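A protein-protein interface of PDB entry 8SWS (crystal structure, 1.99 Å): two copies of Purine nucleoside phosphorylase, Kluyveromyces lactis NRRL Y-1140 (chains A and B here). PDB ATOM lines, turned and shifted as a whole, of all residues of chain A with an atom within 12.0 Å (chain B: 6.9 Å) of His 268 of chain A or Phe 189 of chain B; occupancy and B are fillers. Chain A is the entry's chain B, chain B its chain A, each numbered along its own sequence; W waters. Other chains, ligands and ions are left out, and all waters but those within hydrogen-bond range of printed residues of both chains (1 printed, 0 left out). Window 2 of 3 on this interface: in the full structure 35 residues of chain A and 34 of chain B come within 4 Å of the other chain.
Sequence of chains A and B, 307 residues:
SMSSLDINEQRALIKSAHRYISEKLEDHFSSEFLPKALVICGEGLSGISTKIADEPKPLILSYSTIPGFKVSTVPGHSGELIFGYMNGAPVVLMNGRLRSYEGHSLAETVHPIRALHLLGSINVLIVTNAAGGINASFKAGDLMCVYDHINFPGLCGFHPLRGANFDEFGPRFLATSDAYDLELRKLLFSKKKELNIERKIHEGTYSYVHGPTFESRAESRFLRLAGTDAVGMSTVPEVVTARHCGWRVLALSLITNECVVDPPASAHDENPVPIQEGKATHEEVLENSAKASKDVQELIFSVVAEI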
ATOM      1  N   PRO A 263     -23.458 -19.803  -1.022  1.00  0.00           N
ATOM      2  CA  PRO A 263     -22.153 -19.162  -1.311  1.00  0.00           C
ATOM      3  C   PRO A 263     -21.078 -20.221  -1.531  1.00  0.00           C
ATOM      4  O   PRO A 263     -21.083 -21.293  -0.877  1.00  0.00           O
ATOM      5  CB  PRO A 263     -21.875 -18.339  -0.043  1.00  0.00           C
ATOM      6  CG  PRO A 263     -23.297 -18.002   0.478  1.00  0.00           C
ATOM      7  CD  PRO A 263     -24.102 -19.264   0.195  1.00  0.00           C
ATOM      8  N   PRO A 264     -20.123 -19.954  -2.424  1.00  0.00           N
ATOM      9  CA  PRO A 264     -19.046 -20.923  -2.671  1.00  0.00           C
ATOM     10  C   PRO A 264     -18.113 -21.001  -1.470  1.00  0.00           C
ATOM     11  O   PRO A 264     -18.038 -20.085  -0.652  1.00  0.00           O
ATOM     12  CB  PRO A 264     -18.296 -20.320  -3.860  1.00  0.00           C
ATOM     13  CG  PRO A 264     -18.470 -18.803  -3.644  1.00  0.00           C
ATOM     14  CD  PRO A 264     -19.795 -18.607  -2.936  1.00  0.00           C
ATOM     15  N   ALA A 265     -17.341 -22.084  -1.426  1.00  0.00           N
ATOM     16  CA  ALA A 265     -16.344 -22.255  -0.376  1.00  0.00           C
ATOM     17  C   ALA A 265     -15.436 -21.039  -0.285  1.00  0.00           C
ATOM     18  O   ALA A 265     -14.954 -20.535  -1.296  1.00  0.00           O
ATOM     19  CB  ALA A 265     -15.499 -23.495  -0.665  1.00  0.00           C
ATOM     20  N   SER A 266     -15.207 -20.581   0.941  1.00  0.00           N
ATOM     21  CA  SER A 266     -14.247 -19.534   1.228  1.00  0.00           C
ATOM     22  C   SER A 266     -12.817 -20.064   1.223  1.00  0.00           C
ATOM     23  O   SER A 266     -12.546 -21.202   1.622  1.00  0.00           O
ATOM     24  CB  SER A 266     -14.538 -18.941   2.605  1.00  0.00           C
ATOM     25  OG  SER A 266     -13.450 -18.171   3.033  1.00  0.00           O
ATOM     26  N   ALA A 267     -11.878 -19.192   0.847  1.00  0.00           N
ATOM     27  CA  ALA A 267     -10.472 -19.551   0.915  1.00  0.00           C
ATOM     28  C   ALA A 267     -10.016 -19.771   2.349  1.00  0.00           C
ATOM     29  O   ALA A 267      -8.981 -20.419   2.571  1.00  0.00           O
ATOM     30  CB  ALA A 267      -9.611 -18.462   0.259  1.00  0.00           C
ATOM     31  N   HIS A 268     -10.752 -19.232   3.322  1.00  0.00           N
ATOM     32  CA  HIS A 268     -10.439 -19.413   4.738  1.00  0.00           C
ATOM     33  C   HIS A 268     -11.098 -20.644   5.343  1.00  0.00           C
ATOM     34  O   HIS A 268     -10.914 -20.878   6.541  1.00  0.00           O
ATOM     35  CB  HIS A 268     -10.883 -18.180   5.530  1.00  0.00           C
ATOM     36  CG  HIS A 268     -10.440 -16.901   4.916  1.00  0.00           C
ATOM     37  ND1 HIS A 268      -9.108 -16.602   4.716  1.00  0.00           N
ATOM     38  CD2 HIS A 268     -11.143 -15.957   4.248  1.00  0.00           C
ATOM     39  CE1 HIS A 268      -9.015 -15.440   4.091  1.00  0.00           C
ATOM     40  NE2 HIS A 268     -10.236 -15.044   3.766  1.00  0.00           N
ATOM     41  N   ASP A 269     -11.863 -21.423   4.572  1.00  0.00           N
ATOM     42  CA  ASP A 269     -12.541 -22.594   5.129  1.00  0.00           C
ATOM     43  C   ASP A 269     -11.556 -23.741   5.250  1.00  0.00           C
ATOM     44  O   ASP A 269     -11.018 -24.187   4.234  1.00  0.00           O
ATOM     45  CB  ASP A 269     -13.693 -23.072   4.248  1.00  0.00           C
ATOM     46  CG  ASP A 269     -14.858 -22.122   4.248  1.00  0.00           C
ATOM     47  OD1 ASP A 269     -14.875 -21.247   5.149  1.00  0.00           O
ATOM     48  OD2 ASP A 269     -15.757 -22.255   3.358  1.00  0.00           O
ATOM     49  N   GLU A 270     -11.376 -24.295   6.447  1.00  0.00           N
ATOM     50  CA  GLU A 270     -10.510 -25.466   6.446  1.00  0.00           C
ATOM     51  C   GLU A 270     -11.237 -26.743   6.052  1.00  0.00           C
ATOM     52  O   GLU A 270     -10.568 -27.753   5.805  1.00  0.00           O
ATOM     53  CB  GLU A 270      -9.814 -25.652   7.794  1.00  0.00           C
ATOM     54  CG  GLU A 270     -10.693 -25.522   9.007  1.00  0.00           C
ATOM     55  CD  GLU A 270     -10.042 -26.107  10.244  1.00  0.00           C
ATOM     56  OE1 GLU A 270      -9.018 -25.530  10.720  1.00  0.00           O
ATOM     57  OE2 GLU A 270     -10.549 -27.168  10.722  1.00  0.00           O
ATOM     58  N   ASN A 271     -12.563 -26.737   5.982  1.00  0.00           N
ATOM     59  CA  ASN A 271     -13.340 -27.915   5.596  1.00  0.00           C
ATOM     60  C   ASN A 271     -14.346 -27.534   4.534  1.00  0.00           C
ATOM     61  O   ASN A 271     -15.554 -27.596   4.772  1.00  0.00           O
ATOM     62  CB  ASN A 271     -14.063 -28.524   6.798  1.00  0.00           C
ATOM     63  CG  ASN A 271     -13.117 -28.952   7.866  1.00  0.00           C
ATOM     64  OD1 ASN A 271     -12.928 -28.255   8.857  1.00  0.00           O
ATOM     65  ND2 ASN A 271     -12.527 -30.119   7.691  1.00  0.00           N
ATOM     66  N   PRO A 272     -13.877 -27.107   3.352  1.00  0.00           N
ATOM     67  CA  PRO A 272     -14.780 -26.516   2.361  1.00  0.00           C
ATOM     68  C   PRO A 272     -15.591 -27.559   1.615  1.00  0.00           C
ATOM     69  O   PRO A 272     -15.147 -28.683   1.369  1.00  0.00           O
ATOM     70  CB  PRO A 272     -13.830 -25.799   1.392  1.00  0.00           C
ATOM     71  CG  PRO A 272     -12.509 -26.535   1.509  1.00  0.00           C
ATOM     72  CD  PRO A 272     -12.467 -27.151   2.894  1.00  0.00           C
ATOM     73  N   VAL A 273     -16.803 -27.161   1.254  1.00  0.00           N
ATOM     74  CA  VAL A 273     -17.608 -27.871   0.271  1.00  0.00           C
ATOM     75  C   VAL A 273     -16.994 -27.582  -1.094  1.00  0.00           C
ATOM     76  O   VAL A 273     -16.840 -26.414  -1.445  1.00  0.00           O
ATOM     77  CB  VAL A 273     -19.078 -27.417   0.333  1.00  0.00           C
ATOM     78  CG1 VAL A 273     -19.917 -28.198  -0.680  1.00  0.00           C
ATOM     79  CG2 VAL A 273     -19.628 -27.593   1.766  1.00  0.00           C
ATOM     80  N   ILE A 275     -16.447 -26.566  -4.865  1.00  0.00           N
ATOM     81  CA  ILE A 275     -17.309 -25.649  -5.597  1.00  0.00           C
ATOM     82  C   ILE A 275     -18.019 -26.353  -6.740  1.00  0.00           C
ATOM     83  O   ILE A 275     -19.052 -25.861  -7.207  1.00  0.00           O
ATOM     84  CB  ILE A 275     -16.558 -24.418  -6.141  1.00  0.00           C
ATOM     85  CG1 ILE A 275     -15.458 -24.839  -7.115  1.00  0.00           C
ATOM     86  CG2 ILE A 275     -15.950 -23.588  -4.972  1.00  0.00           C
ATOM     87  CD1 ILE A 275     -14.711 -23.639  -7.678  1.00  0.00           C
ATOM     88  N   MET B 144     -10.692  -7.139  -3.390  1.00  0.00           N
ATOM     89  CA  MET B 144     -11.671  -8.223  -3.256  1.00  0.00           C
ATOM     90  C   MET B 144     -11.277  -9.355  -4.187  1.00  0.00           C
ATOM     91  O   MET B 144     -11.302  -9.194  -5.417  1.00  0.00           O
ATOM     92  CB  MET B 144     -13.087  -7.787  -3.599  1.00  0.00           C
ATOM     93  CG  MET B 144     -14.151  -8.853  -3.267  1.00  0.00           C
ATOM     94  SD  MET B 144     -15.782  -8.412  -3.951  1.00  0.00           S
ATOM     95  CE  MET B 144     -15.537  -8.864  -5.664  1.00  0.00           C
ATOM     96  N   CYS B 145     -10.894 -10.476  -3.605  1.00  0.00           N
ATOM     97  CA  CYS B 145     -10.856 -11.722  -4.353  1.00  0.00           C
ATOM     98  C   CYS B 145     -12.278 -12.107  -4.769  1.00  0.00           C
ATOM     99  O   CYS B 145     -13.166 -12.272  -3.909  1.00  0.00           O
ATOM    100  CB  CYS B 145     -10.229 -12.826  -3.483  1.00  0.00           C
ATOM    101  SG  CYS B 145     -10.005 -14.396  -4.421  1.00  0.00           S
ATOM    102  N   LEU B 182     -11.055 -22.723  -6.009  1.00  0.00           N
ATOM    103  CA  LEU B 182     -10.725 -22.521  -4.596  1.00  0.00           C
ATOM    104  C   LEU B 182      -9.222 -22.534  -4.353  1.00  0.00           C
ATOM    105  O   LEU B 182      -8.708 -21.667  -3.650  1.00  0.00           O
ATOM    106  CB  LEU B 182     -11.429 -23.573  -3.747  1.00  0.00           C
ATOM    107  CG  LEU B 182     -11.157 -23.464  -2.218  1.00  0.00           C
ATOM    108  CD1 LEU B 182     -11.639 -22.143  -1.599  1.00  0.00           C
ATOM    109  CD2 LEU B 182     -11.744 -24.648  -1.510  1.00  0.00           C
ATOM    110  N   LEU B 184      -6.782 -21.668  -6.237  1.00  0.00           N
ATOM    111  CA  LEU B 184      -6.146 -20.407  -6.627  1.00  0.00           C
ATOM    112  C   LEU B 184      -6.433 -19.282  -5.632  1.00  0.00           C
ATOM    113  O   LEU B 184      -5.578 -18.421  -5.400  1.00  0.00           O
ATOM    114  CB  LEU B 184      -6.586 -19.999  -8.050  1.00  0.00           C
ATOM    115  CG  LEU B 184      -6.066 -20.875  -9.190  1.00  0.00           C
ATOM    116  CD1 LEU B 184      -6.602 -20.353 -10.567  1.00  0.00           C
ATOM    117  CD2 LEU B 184      -4.538 -20.936  -9.211  1.00  0.00           C
ATOM    118  N   ARG B 185      -7.638 -19.216  -5.082  1.00  0.00           N
ATOM    119  CA  ARG B 185      -7.907 -18.195  -4.068  1.00  0.00           C
ATOM    120  C   ARG B 185      -7.106 -18.476  -2.803  1.00  0.00           C
ATOM    121  O   ARG B 185      -6.617 -17.550  -2.120  1.00  0.00           O
ATOM    122  CB  ARG B 185      -9.415 -18.173  -3.786  1.00  0.00           C
ATOM    123  CG  ARG B 185     -10.217 -17.596  -4.990  1.00  0.00           C
ATOM    124  CD  ARG B 185     -11.746 -17.440  -4.726  1.00  0.00           C
ATOM    125  NE  ARG B 185     -12.426 -18.737  -4.837  1.00  0.00           N
ATOM    126  CZ  ARG B 185     -13.050 -19.356  -3.841  1.00  0.00           C
ATOM    127  NH1 ARG B 185     -13.013 -18.889  -2.600  1.00  0.00           N
ATOM    128  NH2 ARG B 185     -13.720 -20.478  -4.093  1.00  0.00           N
ATOM    129  N   LYS B 186      -6.911 -19.755  -2.497  1.00  0.00           N
ATOM    130  CA  LYS B 186      -6.094 -20.069  -1.334  1.00  0.00           C
ATOM    131  C   LYS B 186      -4.645 -19.675  -1.597  1.00  0.00           C
ATOM    132  O   LYS B 186      -3.972 -19.131  -0.707  1.00  0.00           O
ATOM    133  CB  LYS B 186      -6.243 -21.554  -0.985  1.00  0.00           C
ATOM    134  CG  LYS B 186      -7.637 -21.893  -0.314  1.00  0.00           C
ATOM    135  CD  LYS B 186      -7.672 -23.375   0.145  1.00  0.00           C
ATOM    136  CE  LYS B 186      -8.159 -23.578   1.605  1.00  0.00           C
ATOM    137  NZ  LYS B 186      -9.674 -23.473   1.756  1.00  0.00           N
ATOM    138  N   LEU B 187      -4.165 -19.907  -2.832  1.00  0.00           N
ATOM    139  CA  LEU B 187      -2.799 -19.530  -3.193  1.00  0.00           C
ATOM    140  C   LEU B 187      -2.592 -18.021  -3.101  1.00  0.00           C
ATOM    141  O   LEU B 187      -1.550 -17.564  -2.624  1.00  0.00           O
ATOM    142  CB  LEU B 187      -2.462 -20.041  -4.607  1.00  0.00           C
ATOM    143  CG  LEU B 187      -1.152 -19.539  -5.223  1.00  0.00           C
ATOM    144  CD1 LEU B 187       0.092 -20.089  -4.468  1.00  0.00           C
ATOM    145  CD2 LEU B 187      -1.092 -19.987  -6.667  1.00  0.00           C
ATOM    146  N   LEU B 188      -3.583 -17.234  -3.541  1.00  0.00           N
ATOM    147  CA  LEU B 188      -3.513 -15.776  -3.415  1.00  0.00           C
ATOM    148  C   LEU B 188      -3.382 -15.353  -1.958  1.00  0.00           C
ATOM    149  O   LEU B 188      -2.511 -14.545  -1.597  1.00  0.00           O
ATOM    150  CB  LEU B 188      -4.758 -15.146  -4.058  1.00  0.00           C
ATOM    151  CG  LEU B 188      -4.870 -13.621  -3.947  1.00  0.00           C
ATOM    152  CD1 LEU B 188      -3.785 -12.927  -4.796  1.00  0.00           C
ATOM    153  CD2 LEU B 188      -6.276 -13.173  -4.374  1.00  0.00           C
ATOM    154  N   PHE B 189      -4.222 -15.915  -1.091  1.00  0.00           N
ATOM    155  CA  PHE B 189      -4.115 -15.558   0.316  1.00  0.00           C
ATOM    156  C   PHE B 189      -2.779 -16.010   0.905  1.00  0.00           C
ATOM    157  O   PHE B 189      -2.182 -15.291   1.712  1.00  0.00           O
ATOM    158  CB  PHE B 189      -5.303 -16.133   1.066  1.00  0.00           C
ATOM    159  CG  PHE B 189      -6.542 -15.309   0.898  1.00  0.00           C
ATOM    160  CD1 PHE B 189      -6.726 -14.158   1.653  1.00  0.00           C
ATOM    161  CD2 PHE B 189      -7.499 -15.647  -0.071  1.00  0.00           C
ATOM    162  CE1 PHE B 189      -7.879 -13.383   1.476  1.00  0.00           C
ATOM    163  CE2 PHE B 189      -8.648 -14.867  -0.253  1.00  0.00           C
ATOM    164  CZ  PHE B 189      -8.829 -13.732   0.515  1.00  0.00           C
ATOM    165  N   SER B 190      -2.273 -17.182   0.488  1.00  0.00           N
ATOM    166  CA  SER B 190      -0.950 -17.622   0.931  1.00  0.00           C
ATOM    167  C   SER B 190       0.137 -16.628   0.543  1.00  0.00           C
ATOM    168  O   SER B 190       1.127 -16.452   1.283  1.00  0.00           O
ATOM    169  CB  SER B 190      -0.613 -18.980   0.336  1.00  0.00           C
ATOM    170  OG  SER B 190      -1.217 -20.005   1.073  1.00  0.00           O
ATOM    171  N   LYS B 191       0.015 -16.017  -0.639  1.00  0.00           N
ATOM    172  CA  LYS B 191       1.059 -15.085  -1.039  1.00  0.00           C
ATOM    173  C   LYS B 191       0.889 -13.744  -0.334  1.00  0.00           C
ATOM    174  O   LYS B 191       1.883 -13.103   0.002  1.00  0.00           O
ATOM    175  CB  LYS B 191       1.099 -14.920  -2.571  1.00  0.00           C
ATOM    176  CG  LYS B 191       1.299 -16.250  -3.321  1.00  0.00           C
ATOM    177  CD  LYS B 191       2.676 -16.930  -3.087  1.00  0.00           C
ATOM    178  CE  LYS B 191       2.590 -18.002  -1.950  1.00  0.00           C
ATOM    179  NZ  LYS B 191       3.866 -18.788  -1.750  1.00  0.00           N
ATOM    180  N   LYS B 192      -0.346 -13.320  -0.054  1.00  0.00           N
ATOM    181  CA  LYS B 192      -0.507 -12.149   0.797  1.00  0.00           C
ATOM    182  C   LYS B 192       0.198 -12.351   2.134  1.00  0.00           C
ATOM    183  O   LYS B 192       0.894 -11.445   2.619  1.00  0.00           O
ATOM    184  CB  LYS B 192      -1.984 -11.862   1.022  1.00  0.00           C
ATOM    185  CG  LYS B 192      -2.185 -10.718   1.983  1.00  0.00           C
ATOM    186  CD  LYS B 192      -3.651 -10.522   2.368  1.00  0.00           C
ATOM    187  CE  LYS B 192      -3.663  -9.786   3.713  1.00  0.00           C
ATOM    188  NZ  LYS B 192      -4.939  -9.108   4.028  1.00  0.00           N
ATOM    189  N   LYS B 193       0.046 -13.549   2.735  1.00  0.00           N
ATOM    190  CA  LYS B 193       0.765 -13.885   3.965  1.00  0.00           C
ATOM    191  C   LYS B 193       2.276 -13.837   3.765  1.00  0.00           C
ATOM    192  O   LYS B 193       2.997 -13.191   4.538  1.00  0.00           O
ATOM    193  CB  LYS B 193       0.372 -15.282   4.460  1.00  0.00           C
ATOM    194  CG  LYS B 193       1.066 -15.670   5.793  1.00  0.00           C
ATOM    195  CD  LYS B 193       0.419 -16.928   6.376  1.00  0.00           C
ATOM    196  CE  LYS B 193       1.064 -17.369   7.719  1.00  0.00           C
ATOM    197  NZ  LYS B 193       0.049 -17.463   8.805  1.00  0.00           N
ATOM    198  N   GLU B 194       2.780 -14.580   2.765  1.00  0.00           N
ATOM    199  CA  GLU B 194       4.225 -14.672   2.555  1.00  0.00           C
ATOM    200  C   GLU B 194       4.838 -13.293   2.319  1.00  0.00           C
ATOM    201  O   GLU B 194       5.960 -13.026   2.753  1.00  0.00           O
ATOM    202  CB  GLU B 194       4.529 -15.587   1.365  1.00  0.00           C
ATOM    203  CG  GLU B 194       5.986 -15.489   0.876  1.00  0.00           C
ATOM    204  CD  GLU B 194       6.275 -16.408  -0.299  1.00  0.00           C
ATOM    205  OE1 GLU B 194       5.301 -16.836  -0.936  1.00  0.00           O
ATOM    206  OE2 GLU B 194       7.472 -16.651  -0.603  1.00  0.00           O
ATOM    207  N   LYS B 200      -6.241  -5.036   2.888  1.00  0.00           N
ATOM    208  CA  LYS B 200      -7.316  -6.027   2.967  1.00  0.00           C
ATOM    209  C   LYS B 200      -7.538  -6.729   1.636  1.00  0.00           C
ATOM    210  O   LYS B 200      -7.431  -6.136   0.558  1.00  0.00           O
ATOM    211  CB  LYS B 200      -8.644  -5.409   3.402  1.00  0.00           C
ATOM    212  CG  LYS B 200      -8.588  -4.802   4.754  1.00  0.00           C
ATOM    213  CD  LYS B 200      -9.815  -4.010   5.042  1.00  0.00           C
ATOM    214  CE  LYS B 200      -9.661  -3.331   6.398  1.00  0.00           C
ATOM    215  NZ  LYS B 200     -10.952  -3.457   7.140  1.00  0.00           N
ATOM    216  N   ILE B 201      -7.867  -8.006   1.717  1.00  0.00           N
ATOM    217  CA  ILE B 201      -8.338  -8.749   0.571  1.00  0.00           C
ATOM    218  C   ILE B 201      -9.618  -9.403   1.049  1.00  0.00           C
ATOM    219  O   ILE B 201      -9.572 -10.360   1.839  1.00  0.00           O
ATOM    220  CB  ILE B 201      -7.328  -9.783   0.062  1.00  0.00           C
ATOM    221  CG1 ILE B 201      -5.997  -9.095  -0.294  1.00  0.00           C
ATOM    222  CG2 ILE B 201      -7.918 -10.568  -1.142  1.00  0.00           C
ATOM    223  CD1 ILE B 201      -4.962 -10.020  -0.889  1.00  0.00           C
ATOM    224  N   HIS B 202     -10.760  -8.843   0.644  1.00  0.00           N
ATOM    225  CA  HIS B 202     -12.049  -9.483   0.889  1.00  0.00           C
ATOM    226  C   HIS B 202     -12.257 -10.653  -0.070  1.00  0.00           C
ATOM    227  O   HIS B 202     -11.455 -10.913  -0.973  1.00  0.00           O
ATOM    228  CB  HIS B 202     -13.216  -8.492   0.724  1.00  0.00           C
ATOM    229  CG  HIS B 202     -13.066  -7.216   1.504  1.00  0.00           C
ATOM    230  ND1 HIS B 202     -13.498  -7.094   2.808  1.00  0.00           N
ATOM    231  CD2 HIS B 202     -12.606  -5.992   1.145  1.00  0.00           C
ATOM    232  CE1 HIS B 202     -13.277  -5.861   3.229  1.00  0.00           C
ATOM    233  NE2 HIS B 202     -12.732  -5.173   2.242  1.00  0.00           N
ATOM    234  N   GLU B 203     -13.375 -11.346   0.120  1.00  0.00           N
ATOM    235  CA  GLU B 203     -13.933 -12.300  -0.826  1.00  0.00           C
ATOM    236  C   GLU B 203     -15.360 -11.858  -1.086  1.00  0.00           C
ATOM    237  O   GLU B 203     -16.106 -11.613  -0.127  1.00  0.00           O
ATOM    238  CB  GLU B 203     -13.943 -13.725  -0.247  1.00  0.00           C
ATOM    239  CG  GLU B 203     -12.720 -14.540  -0.516  1.00  0.00           C
ATOM    240  CD  GLU B 203     -12.892 -15.973  -0.039  1.00  0.00           C
ATOM    241  OE1 GLU B 203     -13.533 -16.178   1.036  1.00  0.00           O
ATOM    242  OE2 GLU B 203     -12.410 -16.886  -0.742  1.00  0.00           O
ATOM    243  N   LEU B 299       1.624  -9.569  -5.739  1.00  0.00           N
ATOM    244  CA  LEU B 299       0.789 -10.752  -5.538  1.00  0.00           C
ATOM    245  C   LEU B 299       0.802 -11.639  -6.780  1.00  0.00           C
ATOM    246  O   LEU B 299       0.937 -12.866  -6.678  1.00  0.00           O
ATOM    247  CB  LEU B 299      -0.644 -10.332  -5.193  1.00  0.00           C
ATOM    248  CG  LEU B 299      -0.804  -9.795  -3.764  1.00  0.00           C
ATOM    249  CD1 LEU B 299      -2.083  -8.976  -3.551  1.00  0.00           C
ATOM    250  CD2 LEU B 299      -0.743 -11.002  -2.750  1.00  0.00           C
ATOM    251  N   VAL B 303       2.196 -15.467  -7.424  1.00  0.00           N
ATOM    252  CA  VAL B 303       1.243 -16.505  -7.797  1.00  0.00           C
ATOM    253  C   VAL B 303       1.747 -17.292  -9.006  1.00  0.00           C
ATOM    254  O   VAL B 303       1.685 -18.529  -9.027  1.00  0.00           O
ATOM    255  CB  VAL B 303      -0.138 -15.874  -8.056  1.00  0.00           C
ATOM    256  CG1 VAL B 303      -1.041 -16.812  -8.895  1.00  0.00           C
ATOM    257  CG2 VAL B 303      -0.823 -15.552  -6.727  1.00  0.00           C
HETATM  258  O   HOH W   1     -11.126 -12.423   2.987  1.00  0.00           O
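Among the printed residues, pairs that only touch across the chains: Ser 266 of chain A with Leu 182 of chain B, His 268 of chain A with Phe 189 of chain B, Ala 267 of chain A with Phe 189 of chain B, Pro 272 of chain A with Leu 182 of chain B, Ala 267 of chain A with Arg 185 of chain B, Ser 266 of chain A with Lys 186 of chain B, Ala 265 of chain A with Leu 182 of chain B, Ala 267 of chain A with Leu 182 of chain B and Ile 275 of chain A with Arg 185 of chain B.
Printed residues of chain B within 4 Å of Ser 266 of chain A: Leu 182 (3.5 Å), Lys 186 (3.7 Å) and Glu 203 (2.8 Å). Of the printed residues of chain B, Ala 267 of chain A touches Leu 182 (3.8 Å), Arg 185 (3.6 Å), Lys 186 (3.2 Å), Phe 189 (3.5 Å) and Glu 203 (2.9 Å). Of the printed residues of chain B, His 268 of chain A touches Phe 189 (3.5 Å). Asn 271 of chain A touches none of the printed residues of chain B. Printed residues of chain B within 4 Å of Ile 275 of chain A: Arg 185. No residue of chain A comes within 4 Å of Cys 145 of chain B. Of the printed residues of chain A, Arg 185 of chain B touches Ala 265, Ala 267 and Ile 275. Lys 186 of chain B touches just these residues of chain A: Ser 266, Ala 267 and Asp 269. No residue of chain A comes within 4 Å of Leu 187 of chain B. No residue of chain A comes within 4 Å of Leu 188 of chain B. Phe 189 of chain B touches two residues of chain A. No residue of chain A comes within 4 Å of Ser 190 of chain B. No residue of chain A comes within 4 Å of Lys 191 of chain B. Lys 193 of chain B touches none of the printed residues of chain A. His 202 of chain B touches none of the printed residues of chain A. Printed residues of chain A within 4 Å of Glu 203 of chain B: Ser 266 (2.8 Å) and Ala 267 (2.9 Å). The nearest printed residue of chain A that does not touch Leu 182 of chain B is Ile 275 of chain A (4.1 Å).
The guanidinium group of Arg 185 of chain B is in salt-bridge range of the side-chain carboxylate of Glu 203 of chain B (2.8 Å). N of Ser 266 of chain A lies within hydrogen-bond range of OD2 of Asp 269 of chain A (3.0 Å). OG of Ser 266 of chain A sits at hydrogen-bond distance from N of His 268 of chain A, 2.9 Å away. The backbone carbonyl oxygen (O) of Lys 186 of chain B lies within hydrogen-bond range of the side-chain hydroxyl (OG) of Ser 190 of chain B (3.4 Å).
The side-chain carboxylate of Glu 203 of chain B lies within hydrogen-bond range of the backbone NH of Ala 267 of chain A, 2.9 Å away. The side-chain amino group of Lys 186 of chain B sits at hydrogen-bond distance from the backbone carbonyl oxygen of Ala 267 of chain A, at 3.2 Å. The guanidinium group (NH1) of Arg 185 of chain B lies within hydrogen-bond range of the backbone carbonyl oxygen (O) of Ala 265 of chain A. The backbone carbonyl oxygen of Asp 269 of chain A is in hydrogen-bond range of the side-chain amino group of Lys 186 of chain B (2.9 Å). OE1 of Glu 203 of chain B sits at hydrogen-bond distance from OG of Ser 266 of chain A (2.8 Å).
No position is printed for both chains. Of the 14 pairs that touch across the chains among the printed residues, none has its exchanged pair printed and touching as well.
Water W1 lies within hydrogen-bond range of the backbone carbonyl oxygen of Ile 201 of chain B (2.8 Å) and a ring nitrogen (NE2) of His 268 of chain A (2.9 Å).
Of the 12 printed residues of chain A, 7 touch a printed residue of chain B. Printed residues of chain A that touch a printed residue of chain B: Ala 265, Ser 266, Ala 267, His 268, Asp 269, Pro 272 and Ile 275. Printed residues of chain B that touch a printed residue of chain A: Leu 182, Arg 185, Lys 186, Phe 189 and Glu 203. Hydrophobic or aromatic side chains of chain B that line the printed part of chain A: Leu 182 and Phe 189.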
